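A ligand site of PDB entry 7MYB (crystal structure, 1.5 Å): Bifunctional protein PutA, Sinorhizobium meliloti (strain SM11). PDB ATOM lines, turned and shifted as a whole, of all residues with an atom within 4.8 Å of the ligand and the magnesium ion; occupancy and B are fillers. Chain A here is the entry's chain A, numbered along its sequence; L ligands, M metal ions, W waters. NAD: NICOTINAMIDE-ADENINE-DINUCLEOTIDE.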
ATOM      1  N   ILE A 705       5.037   1.646  14.000  1.00  0.00           N
ATOM      2  CA  ILE A 705       4.339   1.053  12.876  1.00  0.00           C
ATOM      3  C   ILE A 705       4.994   1.572  11.615  1.00  0.00           C
ATOM      4  O   ILE A 705       5.138   2.795  11.442  1.00  0.00           O
ATOM      5  CB  ILE A 705       2.834   1.373  12.912  1.00  0.00           C
ATOM      6  CG1 ILE A 705       2.175   0.697  14.112  1.00  0.00           C
ATOM      7  CG2 ILE A 705       2.154   0.940  11.648  1.00  0.00           C
ATOM      8  CD1 ILE A 705       0.867   1.359  14.518  1.00  0.00           C
ATOM      9  N   SER A 706       5.414   0.659  10.736  1.00  0.00           N
ATOM     10  CA  SER A 706       6.289   1.021   9.640  1.00  0.00           C
ATOM     11  C   SER A 706       5.748   0.536   8.307  1.00  0.00           C
ATOM     12  O   SER A 706       4.961  -0.409   8.250  1.00  0.00           O
ATOM     13  CB  SER A 706       7.707   0.453   9.884  1.00  0.00           C
ATOM     14  OG  SER A 706       7.679  -0.914  10.190  1.00  0.00           O
ATOM     15  N   PRO A 707       6.186   1.164   7.205  1.00  0.00           N
ATOM     16  CA  PRO A 707       5.669   0.824   5.882  1.00  0.00           C
ATOM     17  C   PRO A 707       6.484  -0.303   5.244  1.00  0.00           C
ATOM     18  O   PRO A 707       7.577  -0.649   5.691  1.00  0.00           O
ATOM     19  CB  PRO A 707       5.870   2.136   5.105  1.00  0.00           C
ATOM     20  CG  PRO A 707       7.115   2.706   5.690  1.00  0.00           C
ATOM     21  CD  PRO A 707       7.052   2.349   7.173  1.00  0.00           C
ATOM     22  N   TRP A 708       5.931  -0.858   4.158  1.00  0.00           N
ATOM     23  CA  TRP A 708       6.646  -1.955   3.485  1.00  0.00           C
ATOM     24  C   TRP A 708       7.791  -1.468   2.617  1.00  0.00           C
ATOM     25  O   TRP A 708       8.731  -2.237   2.374  1.00  0.00           O
ATOM     26  CB  TRP A 708       5.669  -2.804   2.634  1.00  0.00           C
ATOM     27  CG  TRP A 708       5.319  -2.099   1.336  1.00  0.00           C
ATOM     28  CD1 TRP A 708       4.219  -1.327   1.098  1.00  0.00           C
ATOM     29  CD2 TRP A 708       6.097  -2.062   0.125  1.00  0.00           C
ATOM     30  NE1 TRP A 708       4.268  -0.807  -0.171  1.00  0.00           N
ATOM     31  CE2 TRP A 708       5.405  -1.249  -0.792  1.00  0.00           C
ATOM     32  CE3 TRP A 708       7.293  -2.673  -0.271  1.00  0.00           C
ATOM     33  CZ2 TRP A 708       5.885  -0.998  -2.077  1.00  0.00           C
ATOM     34  CZ3 TRP A 708       7.777  -2.414  -1.542  1.00  0.00           C
ATOM     35  CH2 TRP A 708       7.058  -1.606  -2.437  1.00  0.00           C
ATOM     36  N   ASN A 709       7.754  -0.220   2.135  1.00  0.00           N
ATOM     37  CA  ASN A 709       8.593   0.146   0.987  1.00  0.00           C
ATOM     38  C   ASN A 709      10.026   0.470   1.361  1.00  0.00           C
ATOM     39  O   ASN A 709      10.902   0.407   0.491  1.00  0.00           O
ATOM     40  CB  ASN A 709       7.966   1.329   0.257  1.00  0.00           C
ATOM     41  CG  ASN A 709       8.062   2.594   1.054  1.00  0.00           C
ATOM     42  OD1 ASN A 709       7.511   2.684   2.152  1.00  0.00           O
ATOM     43  ND2 ASN A 709       8.762   3.590   0.517  1.00  0.00           N
ATOM     44  N   PHE A 710      10.285   0.851   2.605  1.00  0.00           N
ATOM     45  CA  PHE A 710      11.629   0.955   3.160  1.00  0.00           C
ATOM     46  C   PHE A 710      11.663   0.020   4.359  1.00  0.00           C
ATOM     47  O   PHE A 710      11.665   0.458   5.520  1.00  0.00           O
ATOM     48  CB  PHE A 710      11.990   2.394   3.550  1.00  0.00           C
ATOM     49  CG  PHE A 710      12.007   3.367   2.393  1.00  0.00           C
ATOM     50  CD1 PHE A 710      12.545   3.019   1.166  1.00  0.00           C
ATOM     51  CD2 PHE A 710      11.490   4.641   2.550  1.00  0.00           C
ATOM     52  CE1 PHE A 710      12.564   3.918   0.116  1.00  0.00           C
ATOM     53  CE2 PHE A 710      11.512   5.557   1.498  1.00  0.00           C
ATOM     54  CZ  PHE A 710      12.047   5.187   0.282  1.00  0.00           C
ATOM     55  N   ILE A 714      13.331   2.550   7.505  1.00  0.00           N
ATOM     56  CA  ILE A 714      12.374   3.291   8.338  1.00  0.00           C
ATOM     57  C   ILE A 714      11.998   2.469   9.571  1.00  0.00           C
ATOM     58  O   ILE A 714      11.856   3.007  10.667  1.00  0.00           O
ATOM     59  CB  ILE A 714      11.139   3.687   7.514  1.00  0.00           C
ATOM     60  CG1 ILE A 714      11.553   4.730   6.480  1.00  0.00           C
ATOM     61  CG2 ILE A 714      10.020   4.214   8.431  1.00  0.00           C
ATOM     62  CD1 ILE A 714      10.400   5.408   5.828  1.00  0.00           C
ATOM     63  N   LYS A 732       5.823  -3.130  14.968  1.00  0.00           N
ATOM     64  CA  LYS A 732       4.793  -3.733  14.116  1.00  0.00           C
ATOM     65  C   LYS A 732       5.169  -3.450  12.670  1.00  0.00           C
ATOM     66  O   LYS A 732       4.804  -2.402  12.117  1.00  0.00           O
ATOM     67  CB  LYS A 732       3.407  -3.197  14.458  1.00  0.00           C
ATOM     68  CG  LYS A 732       2.270  -4.196  14.284  1.00  0.00           C
ATOM     69  CD  LYS A 732       2.151  -4.722  12.853  1.00  0.00           C
ATOM     70  CE  LYS A 732       1.691  -3.641  11.867  1.00  0.00           C
ATOM     71  NZ  LYS A 732       1.602  -4.201  10.484  1.00  0.00           N
ATOM     72  N   PRO A 733       5.888  -4.350  12.013  1.00  0.00           N
ATOM     73  CA  PRO A 733       6.268  -4.119  10.618  1.00  0.00           C
ATOM     74  C   PRO A 733       5.103  -4.369   9.668  1.00  0.00           C
ATOM     75  O   PRO A 733       4.145  -5.067   9.981  1.00  0.00           O
ATOM     76  CB  PRO A 733       7.366  -5.158  10.380  1.00  0.00           C
ATOM     77  CG  PRO A 733       6.970  -6.301  11.280  1.00  0.00           C
ATOM     78  CD  PRO A 733       6.352  -5.659  12.511  1.00  0.00           C
ATOM     79  N   ALA A 734       5.225  -3.763   8.477  1.00  0.00           N
ATOM     80  CA  ALA A 734       4.237  -3.973   7.438  1.00  0.00           C
ATOM     81  C   ALA A 734       4.024  -5.464   7.173  1.00  0.00           C
ATOM     82  O   ALA A 734       4.970  -6.266   7.207  1.00  0.00           O
ATOM     83  CB  ALA A 734       4.674  -3.277   6.146  1.00  0.00           C
ATOM     84  N   GLU A 735       2.779  -5.841   6.910  1.00  0.00           N
ATOM     85  CA  GLU A 735       2.468  -7.246   6.661  1.00  0.00           C
ATOM     86  C   GLU A 735       3.199  -7.795   5.430  1.00  0.00           C
ATOM     87  O   GLU A 735       3.458  -8.995   5.347  1.00  0.00           O
ATOM     88  CB  GLU A 735       0.959  -7.440   6.531  1.00  0.00           C
ATOM     89  CG  GLU A 735       0.285  -6.573   5.472  1.00  0.00           C
ATOM     90  CD  GLU A 735      -0.234  -5.244   6.024  1.00  0.00           C
ATOM     91  OE1 GLU A 735       0.306  -4.738   7.038  1.00  0.00           O
ATOM     92  OE2 GLU A 735      -1.178  -4.692   5.420  1.00  0.00           O
ATOM     93  N   GLU A 736       3.556  -6.920   4.478  1.00  0.00           N
ATOM     94  CA  GLU A 736       4.229  -7.368   3.259  1.00  0.00           C
ATOM     95  C   GLU A 736       5.682  -7.769   3.512  1.00  0.00           C
ATOM     96  O   GLU A 736       6.208  -8.617   2.765  1.00  0.00           O
ATOM     97  CB  GLU A 736       4.184  -6.264   2.198  1.00  0.00           C
ATOM     98  CG  GLU A 736       2.789  -5.901   1.705  1.00  0.00           C
ATOM     99  CD  GLU A 736       2.160  -4.752   2.483  1.00  0.00           C
ATOM    100  OE1 GLU A 736       1.190  -4.167   1.956  1.00  0.00           O
ATOM    101  OE2 GLU A 736       2.618  -4.447   3.608  1.00  0.00           O
ATOM    102  N   GLY A 763       2.205  -8.841  11.603  1.00  0.00           N
ATOM    103  CA  GLY A 763       0.791  -8.934  11.297  1.00  0.00           C
ATOM    104  C   GLY A 763       0.334  -7.741  10.473  1.00  0.00           C
ATOM    105  O   GLY A 763       1.135  -6.928  10.025  1.00  0.00           O
ATOM    106  N   ASP A 764      -0.994  -7.648  10.298  1.00  0.00           N
ATOM    107  CA  ASP A 764      -1.561  -6.623   9.445  1.00  0.00           C
ATOM    108  C   ASP A 764      -2.003  -5.412  10.271  1.00  0.00           C
ATOM    109  O   ASP A 764      -1.574  -5.235  11.419  1.00  0.00           O
ATOM    110  CB  ASP A 764      -2.695  -7.227   8.586  1.00  0.00           C
ATOM    111  CG  ASP A 764      -3.822  -7.812   9.412  1.00  0.00           C
ATOM    112  OD1 ASP A 764      -4.015  -7.403  10.576  1.00  0.00           O
ATOM    113  OD2 ASP A 764      -4.537  -8.697   8.894  1.00  0.00           O
ATOM    114  N   GLY A 765      -2.849  -4.561   9.689  1.00  0.00           N
ATOM    115  CA  GLY A 765      -3.254  -3.352  10.375  1.00  0.00           C
ATOM    116  C   GLY A 765      -4.041  -3.593  11.646  1.00  0.00           C
ATOM    117  O   GLY A 765      -4.086  -2.719  12.510  1.00  0.00           O
ATOM    118  N   GLY A 768      -1.464  -3.456  14.362  1.00  0.00           N
ATOM    119  CA  GLY A 768      -1.130  -2.058  14.629  1.00  0.00           C
ATOM    120  C   GLY A 768      -2.201  -1.349  15.427  1.00  0.00           C
ATOM    121  O   GLY A 768      -1.918  -0.627  16.387  1.00  0.00           O
ATOM    122  N   ALA A 769      -3.479  -1.551  15.054  1.00  0.00           N
ATOM    123  CA  ALA A 769      -4.571  -0.860  15.741  1.00  0.00           C
ATOM    124  C   ALA A 769      -4.701  -1.335  17.185  1.00  0.00           C
ATOM    125  O   ALA A 769      -4.955  -0.525  18.092  1.00  0.00           O
ATOM    126  CB  ALA A 769      -5.879  -1.068  14.990  1.00  0.00           C
ATOM    127  N   PHE A 782       4.398   6.458  13.522  1.00  0.00           N
ATOM    128  CA  PHE A 782       3.770   5.896  12.334  1.00  0.00           C
ATOM    129  C   PHE A 782       4.424   6.472  11.091  1.00  0.00           C
ATOM    130  O   PHE A 782       4.568   7.695  10.964  1.00  0.00           O
ATOM    131  CB  PHE A 782       2.269   6.218  12.302  1.00  0.00           C
ATOM    132  CG  PHE A 782       1.597   5.744  11.049  1.00  0.00           C
ATOM    133  CD1 PHE A 782       1.239   4.416  10.912  1.00  0.00           C
ATOM    134  CD2 PHE A 782       1.359   6.604   9.989  1.00  0.00           C
ATOM    135  CE1 PHE A 782       0.620   3.946   9.762  1.00  0.00           C
ATOM    136  CE2 PHE A 782       0.740   6.140   8.830  1.00  0.00           C
ATOM    137  CZ  PHE A 782       0.372   4.817   8.720  1.00  0.00           C
ATOM    138  N   THR A 783       4.765   5.602  10.159  1.00  0.00           N
ATOM    139  CA  THR A 783       5.120   6.003   8.812  1.00  0.00           C
ATOM    140  C   THR A 783       4.307   5.134   7.863  1.00  0.00           C
ATOM    141  O   THR A 783       4.307   3.908   7.983  1.00  0.00           O
ATOM    142  CB  THR A 783       6.632   5.877   8.563  1.00  0.00           C
ATOM    143  OG1 THR A 783       7.331   6.668   9.531  1.00  0.00           O
ATOM    144  CG2 THR A 783       6.976   6.404   7.171  1.00  0.00           C
ATOM    145  N   GLY A 784       3.594   5.773   6.944  1.00  0.00           N
ATOM    146  CA  GLY A 784       2.669   5.043   6.087  1.00  0.00           C
ATOM    147  C   GLY A 784       1.751   6.011   5.355  1.00  0.00           C
ATOM    148  O   GLY A 784       2.074   7.189   5.218  1.00  0.00           O
ATOM    149  N   SER A 785       0.618   5.489   4.917  1.00  0.00           N
ATOM    150  CA  SER A 785      -0.330   6.297   4.145  1.00  0.00           C
ATOM    151  C   SER A 785      -1.069   7.301   5.020  1.00  0.00           C
ATOM    152  O   SER A 785      -1.335   7.068   6.203  1.00  0.00           O
ATOM    153  CB  SER A 785      -1.334   5.393   3.425  1.00  0.00           C
ATOM    154  OG  SER A 785      -2.184   4.707   4.342  1.00  0.00           O
ATOM    155  N   VAL A 788      -4.331   5.892   6.643  1.00  0.00           N
ATOM    156  CA  VAL A 788      -4.169   5.084   7.848  1.00  0.00           C
ATOM    157  C   VAL A 788      -3.790   5.978   9.023  1.00  0.00           C
ATOM    158  O   VAL A 788      -4.295   5.803  10.146  1.00  0.00           O
ATOM    159  CB  VAL A 788      -3.145   3.964   7.615  1.00  0.00           C
ATOM    160  CG1 VAL A 788      -2.777   3.304   8.926  1.00  0.00           C
ATOM    161  CG2 VAL A 788      -3.702   2.939   6.638  1.00  0.00           C
ATOM    162  N   LEU A 791      -6.850   7.263  10.609  1.00  0.00           N
ATOM    163  CA  LEU A 791      -7.499   6.293  11.489  1.00  0.00           C
ATOM    164  C   LEU A 791      -6.801   6.207  12.835  1.00  0.00           C
ATOM    165  O   LEU A 791      -7.458   6.137  13.874  1.00  0.00           O
ATOM    166  CB  LEU A 791      -7.524   4.926  10.815  1.00  0.00           C
ATOM    167  CG  LEU A 791      -8.381   4.814   9.551  1.00  0.00           C
ATOM    168  CD1 LEU A 791      -8.079   3.503   8.848  1.00  0.00           C
ATOM    169  CD2 LEU A 791      -9.843   4.938   9.888  1.00  0.00           C
ATOM    170  N   ILE A 792      -5.461   6.235  12.836  1.00  0.00           N
ATOM    171  CA  ILE A 792      -4.729   6.233  14.101  1.00  0.00           C
ATOM    172  C   ILE A 792      -4.988   7.512  14.888  1.00  0.00           C
ATOM    173  O   ILE A 792      -5.196   7.476  16.107  1.00  0.00           O
ATOM    174  CB  ILE A 792      -3.234   5.995  13.837  1.00  0.00           C
ATOM    175  CG1 ILE A 792      -3.023   4.586  13.290  1.00  0.00           C
ATOM    176  CG2 ILE A 792      -2.389   6.233  15.102  1.00  0.00           C
ATOM    177  CD1 ILE A 792      -1.607   4.338  12.807  1.00  0.00           C
ATOM    178  N   GLN A 795      -8.198   7.032  16.694  1.00  0.00           N
ATOM    179  CA  GLN A 795      -8.027   6.162  17.853  1.00  0.00           C
ATOM    180  C   GLN A 795      -7.429   6.911  19.031  1.00  0.00           C
ATOM    181  O   GLN A 795      -7.887   6.772  20.172  1.00  0.00           O
ATOM    182  CB  GLN A 795      -7.092   4.996  17.520  1.00  0.00           C
ATOM    183  CG  GLN A 795      -7.656   3.833  16.731  1.00  0.00           C
ATOM    184  CD  GLN A 795      -6.628   2.726  16.596  1.00  0.00           C
ATOM    185  OE1 GLN A 795      -5.683   2.830  15.825  1.00  0.00           O
ATOM    186  NE2 GLN A 795      -6.811   1.658  17.368  1.00  0.00           N
ATOM    187  N   GLU A 812       4.272  10.242   9.616  1.00  0.00           N
ATOM    188  CA  GLU A 812       4.992  10.672   8.428  1.00  0.00           C
ATOM    189  C   GLU A 812       4.363   9.962   7.239  1.00  0.00           C
ATOM    190  O   GLU A 812       4.351   8.727   7.194  1.00  0.00           O
ATOM    191  CB  GLU A 812       6.484  10.392   8.586  1.00  0.00           C
ATOM    192  CG  GLU A 812       7.115  11.139   9.784  1.00  0.00           C
ATOM    193  CD  GLU A 812       6.968  12.647   9.676  1.00  0.00           C
ATOM    194  OE1 GLU A 812       7.791  13.276   8.990  1.00  0.00           O
ATOM    195  OE2 GLU A 812       6.027  13.211  10.275  1.00  0.00           O
ATOM    196  N   THR A 813       3.759  10.737   6.331  1.00  0.00           N
ATOM    197  CA  THR A 813       2.804  10.158   5.410  1.00  0.00           C
ATOM    198  C   THR A 813       3.142  10.456   3.939  1.00  0.00           C
ATOM    199  O   THR A 813       4.322  10.632   3.607  1.00  0.00           O
ATOM    200  CB  THR A 813       1.388  10.623   5.793  1.00  0.00           C
ATOM    201  OG1 THR A 813       1.374  12.035   6.061  1.00  0.00           O
ATOM    202  CG2 THR A 813       0.964   9.924   7.084  1.00  0.00           C
ATOM    203  N   GLY A 814       2.143  10.470   3.057  1.00  0.00           N
ATOM    204  CA  GLY A 814       2.420  10.436   1.625  1.00  0.00           C
ATOM    205  C   GLY A 814       2.793  11.788   1.011  1.00  0.00           C
ATOM    206  O   GLY A 814       2.792  12.830   1.657  1.00  0.00           O
ATOM    207  N   GLY A 815       3.088  11.744  -0.290  1.00  0.00           N
ATOM    208  CA  GLY A 815       3.448  12.940  -1.023  1.00  0.00           C
ATOM    209  C   GLY A 815       2.757  12.989  -2.367  1.00  0.00           C
ATOM    210  O   GLY A 815       2.214  11.993  -2.861  1.00  0.00           O
ATOM    211  N   CYS A 846       8.218   7.218  -0.996  1.00  0.00           N
ATOM    212  CA  CYS A 846       7.352   8.319  -0.609  1.00  0.00           C
ATOM    213  C   CYS A 846       7.813   9.628  -1.251  1.00  0.00           C
ATOM    214  O   CYS A 846       6.995  10.513  -1.508  1.00  0.00           O
ATOM    215  CB  CYS A 846       7.309   8.438   0.915  1.00  0.00           C
ATOM    216  SG  CYS A 846       8.907   8.708   1.674  1.00  0.00           S
ATOM    217  N   GLU A 942      -2.307  10.405  -3.854  1.00  0.00           N
ATOM    218  CA  GLU A 942      -1.030   9.779  -4.171  1.00  0.00           C
ATOM    219  C   GLU A 942      -1.249   8.428  -4.850  1.00  0.00           C
ATOM    220  O   GLU A 942      -2.040   7.605  -4.374  1.00  0.00           O
ATOM    221  CB  GLU A 942      -0.233   9.603  -2.878  1.00  0.00           C
ATOM    222  CG  GLU A 942       1.072   8.811  -2.991  1.00  0.00           C
ATOM    223  CD  GLU A 942       1.641   8.461  -1.623  1.00  0.00           C
ATOM    224  OE1 GLU A 942       2.804   8.809  -1.338  1.00  0.00           O
ATOM    225  OE2 GLU A 942       0.907   7.847  -0.808  1.00  0.00           O
ATOM    226  N   PHE A 944       0.907   5.294  -5.693  1.00  0.00           N
ATOM    227  CA  PHE A 944       2.189   4.797  -5.199  1.00  0.00           C
ATOM    228  C   PHE A 944       2.713   3.726  -6.146  1.00  0.00           C
ATOM    229  O   PHE A 944       2.688   2.519  -5.879  1.00  0.00           O
ATOM    230  CB  PHE A 944       2.024   4.266  -3.772  1.00  0.00           C
ATOM    231  CG  PHE A 944       3.294   4.241  -2.965  1.00  0.00           C
ATOM    232  CD1 PHE A 944       3.914   5.435  -2.606  1.00  0.00           C
ATOM    233  CD2 PHE A 944       3.851   3.043  -2.525  1.00  0.00           C
ATOM    234  CE1 PHE A 944       5.090   5.413  -1.849  1.00  0.00           C
ATOM    235  CE2 PHE A 944       5.021   3.033  -1.773  1.00  0.00           C
ATOM    236  CZ  PHE A 944       5.638   4.225  -1.438  1.00  0.00           C
ATOM    237  N   LEU A 972       5.882  17.128   0.724  1.00  0.00           N
ATOM    238  CA  LEU A 972       6.975  16.226   1.085  1.00  0.00           C
ATOM    239  C   LEU A 972       8.256  16.600   0.343  1.00  0.00           C
ATOM    240  O   LEU A 972       9.071  17.362   0.869  1.00  0.00           O
ATOM    241  CB  LEU A 972       6.575  14.767   0.845  1.00  0.00           C
ATOM    242  CG  LEU A 972       7.558  13.731   1.423  1.00  0.00           C
ATOM    243  CD1 LEU A 972       7.918  14.022   2.875  1.00  0.00           C
ATOM    244  CD2 LEU A 972       6.989  12.298   1.284  1.00  0.00           C
ATOM    245  N   PHE A1012      14.625  14.263   6.820  1.00  0.00           N
ATOM    246  CA  PHE A1012      13.574  13.952   5.878  1.00  0.00           C
ATOM    247  C   PHE A1012      12.206  14.009   6.539  1.00  0.00           C
ATOM    248  O   PHE A1012      12.002  13.437   7.615  1.00  0.00           O
ATOM    249  CB  PHE A1012      13.770  12.574   5.234  1.00  0.00           C
ATOM    250  CG  PHE A1012      12.792  12.301   4.150  1.00  0.00           C
ATOM    251  CD1 PHE A1012      13.009  12.801   2.862  1.00  0.00           C
ATOM    252  CD2 PHE A1012      11.619  11.593   4.409  1.00  0.00           C
ATOM    253  CE1 PHE A1012      12.086  12.569   1.844  1.00  0.00           C
ATOM    254  CE2 PHE A1012      10.697  11.357   3.399  1.00  0.00           C
ATOM    255  CZ  PHE A1012      10.933  11.837   2.123  1.00  0.00           C
ATOM    256  N   SER A1018       1.468  15.417   4.318  1.00  0.00           N
ATOM    257  CA  SER A1018       2.684  14.608   4.268  1.00  0.00           C
ATOM    258  C   SER A1018       3.322  14.351   5.627  1.00  0.00           C
ATOM    259  O   SER A1018       4.262  13.566   5.694  1.00  0.00           O
ATOM    260  CB  SER A1018       3.727  15.293   3.376  1.00  0.00           C
ATOM    261  OG  SER A1018       3.249  15.372   2.050  1.00  0.00           O
HETATM  262  PA  NAD L   1       0.150   1.692   4.890  1.00  0.00           P
HETATM  263  O1A NAD L   1      -0.549   2.927   5.387  1.00  0.00           O
HETATM  264  O2A NAD L   1      -0.686   0.873   3.969  1.00  0.00           O
HETATM  265  O5B NAD L   1       0.667   0.762   6.150  1.00  0.00           O
HETATM  266  C5B NAD L   1       1.745   1.233   6.962  1.00  0.00           C
HETATM  267  C4B NAD L   1       1.688   0.409   8.282  1.00  0.00           C
HETATM  268  O4B NAD L   1       0.290   0.745   9.005  1.00  0.00           O
HETATM  269  C3B NAD L   1       1.705  -0.899   8.094  1.00  0.00           C
HETATM  270  O3B NAD L   1       2.528  -1.521   9.189  1.00  0.00           O
HETATM  271  C2B NAD L   1       0.242  -1.369   8.291  1.00  0.00           C
HETATM  272  O2B NAD L   1       0.158  -2.678   8.688  1.00  0.00           O
HETATM  273  C1B NAD L   1      -0.259  -0.421   9.364  1.00  0.00           C
HETATM  274  N9A NAD L   1      -1.692  -0.298   9.221  1.00  0.00           N
HETATM  275  C8A NAD L   1      -2.567  -0.467   8.245  1.00  0.00           C
HETATM  276  N7A NAD L   1      -3.775  -0.178   8.741  1.00  0.00           N
HETATM  277  C5A NAD L   1      -3.631   0.167  10.049  1.00  0.00           C
HETATM  278  C6A NAD L   1      -4.571   0.558  11.021  1.00  0.00           C
HETATM  279  N6A NAD L   1      -6.009   0.635  10.671  1.00  0.00           N
HETATM  280  N1A NAD L   1      -4.158   0.855  12.246  1.00  0.00           N
HETATM  281  C2A NAD L   1      -2.818   0.775  12.576  1.00  0.00           C
HETATM  282  N3A NAD L   1      -1.915   0.395  11.635  1.00  0.00           N
HETATM  283  C4A NAD L   1      -2.337   0.093  10.362  1.00  0.00           C
HETATM  284  O3  NAD L   1       1.515   2.173   4.134  1.00  0.00           O
HETATM  285  PN  NAD L   1       2.583   1.256   3.201  1.00  0.00           P
HETATM  286  O1N NAD L   1       1.785   0.789   1.969  1.00  0.00           O
HETATM  287  O2N NAD L   1       3.226   0.144   3.992  1.00  0.00           O
HETATM  288  O5D NAD L   1       3.736   2.348   2.741  1.00  0.00           O
HETATM  289  C5D NAD L   1       3.442   3.280   1.700  1.00  0.00           C
HETATM  290  C4D NAD L   1       2.942   4.654   2.173  1.00  0.00           C
HETATM  291  O4D NAD L   1       3.941   5.244   3.269  1.00  0.00           O
HETATM  292  C3D NAD L   1       2.941   5.527   1.167  1.00  0.00           C
HETATM  293  O3D NAD L   1       1.716   6.424   1.242  1.00  0.00           O
HETATM  294  C2D NAD L   1       4.172   6.369   1.354  1.00  0.00           C
HETATM  295  O2D NAD L   1       4.052   7.652   0.803  1.00  0.00           O
HETATM  296  C1D NAD L   1       4.232   6.437   2.903  1.00  0.00           C
HETATM  297  N1N NAD L   1       5.644   6.698   3.312  1.00  0.00           N
HETATM  298  C2N NAD L   1       5.986   7.891   3.900  1.00  0.00           C
HETATM  299  C3N NAD L   1       7.314   8.090   4.268  1.00  0.00           C
HETATM  300  C7N NAD L   1       7.763   9.434   4.933  1.00  0.00           C
HETATM  301  O7N NAD L   1       8.859   9.559   5.362  1.00  0.00           O
HETATM  302  N7N NAD L   1       6.789  10.544   4.987  1.00  0.00           N
HETATM  303  C4N NAD L   1       8.242   7.101   4.042  1.00  0.00           C
HETATM  304  C5N NAD L   1       7.886   5.916   3.448  1.00  0.00           C
HETATM  305  C6N NAD L   1       6.563   5.709   3.075  1.00  0.00           C
HETATM  306 MG    MG M   1      -1.494  -0.927   3.357  1.00  0.00          MG
HETATM  307  O   HOH W   1       0.119   4.334  -0.006  1.00  0.00           O
HETATM  308  O   HOH W   2      -4.538  -1.757   6.231  1.00  0.00           O
HETATM  309  O   HOH W   3      -2.311   0.092   1.840  1.00  0.00           O
HETATM  310  O   HOH W   4       6.864  13.303   6.369  1.00  0.00           O
HETATM  311  O   HOH W   5       1.614  -2.121   4.791  1.00  0.00           O
HETATM  312  O   HOH W   6      -0.670   8.773   1.508  1.00  0.00           O
HETATM  313  O   HOH W   7      10.378   9.661   7.537  1.00  0.00           O
HETATM  314  O   HOH W   8      -3.326  -0.312   4.456  1.00  0.00           O
HETATM  315  O   HOH W   9      -0.850  -2.036   5.061  1.00  0.00           O
HETATM  316  O   HOH W  10      -0.702   2.086   1.087  1.00  0.00           O
HETATM  317  O   HOH W  11       0.212  -1.289   2.208  1.00  0.00           O
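Water W11 lies within hydrogen-bond range of an oxygen (O1N) of the ligand (2.6 Å) and the side-chain carboxylate of Glu 736 (3.1 Å). Water W9 lies within hydrogen-bond range of the side-chain carboxylate (OE2) of Glu 735 (2.7 Å) and an oxygen (O5B) of the ligand (3.4 Å). Water W5 lies within hydrogen-bond range of OE2 of Glu 736 (2.8 Å) and O2N of the ligand (2.9 Å). Water W4 lies within hydrogen-bond range of O of Ser 1018 (2.7 Å), OE1 of Glu 812 (2.8 Å) and N7N of the ligand (3.1 Å). Water W6 lies within hydrogen-bond range of the side-chain carboxylate (OE2) of Glu 942 and an oxygen (O3D) of the ligand.
No residue comes within 4 Å of the magnesium ion.
The magnesium ion is bound by water W3 (2.0 Å), O2A of the ligand (2.1 Å), water W11 (2.1 Å), water W9 (2.1 Å) and water W8 (2.2 Å).
O of Thr 813 lies within hydrogen-bond range of N7N of the ligand. N of Ser 785 lies within hydrogen-bond range of O1A of the ligand. OG of Ser 785 lies within hydrogen-bond range of O1A of the ligand (2.6 Å). The side-chain sulfur of Cys 846 sits close to an oxygen (O7N) of the ligand, 3.8 Å away. An oxygen (O3D) of the ligand lies within hydrogen-bond range of the side-chain carboxylate of Glu 942, at 2.6 Å. The backbone NH (N) of Trp 708 is in hydrogen-bond range of an oxygen (O2N) of the ligand (2.9 Å). The backbone carbonyl oxygen (O) of Ser 706 lies within hydrogen-bond range of an oxygen (O3B) of the ligand (2.8 Å). The side-chain carboxylate (OE1) of Glu 735 sits at hydrogen-bond distance from an oxygen (O2B) of the ligand, 2.6 Å away. The side-chain amino group of Lys 732 lies within hydrogen-bond range of an oxygen (O2B) of the ligand, at 2.8 Å.
O4D of the ligand sits close to O of Gly 784 (3.3 Å). Residues that only touch the ligand: Pro 707, Phe 1012, Ile 705, Ile 714, Asn 709, Phe 782, Gly 814, Glu 812, Thr 783, Val 788, Ala 769, Ala 734, Phe 944, Gly 765, Gly 768, Ile 792, Asp 764, Pro 733, Phe 710 and Leu 791. Hydrophobic or aromatic side chains that line the ligand: Ile 705, Pro 707, Trp 708, Phe 710, Ile 714, Ala 769, Phe 782, Val 788, Leu 791, Ile 792, Phe 944 and Phe 1012. Of the 35 residues printed, 29 come within 4 Å of the ligand. Along chain A the residues within 4 Å of the ligand span positions 705 to 1012.
The backbone carbonyl oxygen (O) of Ile 705 lies within hydrogen-bond range of the backbone NH (N) of Thr 783, at 3.1 Å. NZ of Lys 732 is in salt-bridge range of OE1 of Glu 735 (3.7 Å). O of Ser 706 lies within hydrogen-bond range of N of Ala 734. O of Asp 764 is in hydrogen-bond range of NZ of Lys 732. The backbone carbonyl oxygen of Gly 763 sits at hydrogen-bond distance from the side-chain amino group of Lys 732 (2.8 Å). O of Phe 782 is in hydrogen-bond range of N of Glu 812 (2.9 Å). O of Ala 769 is in hydrogen-bond range of NE2 of Gln 795, at 3.0 Å. The backbone NH (N) of Gly 784 lies within hydrogen-bond range of the backbone carbonyl oxygen (O) of Glu 812.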
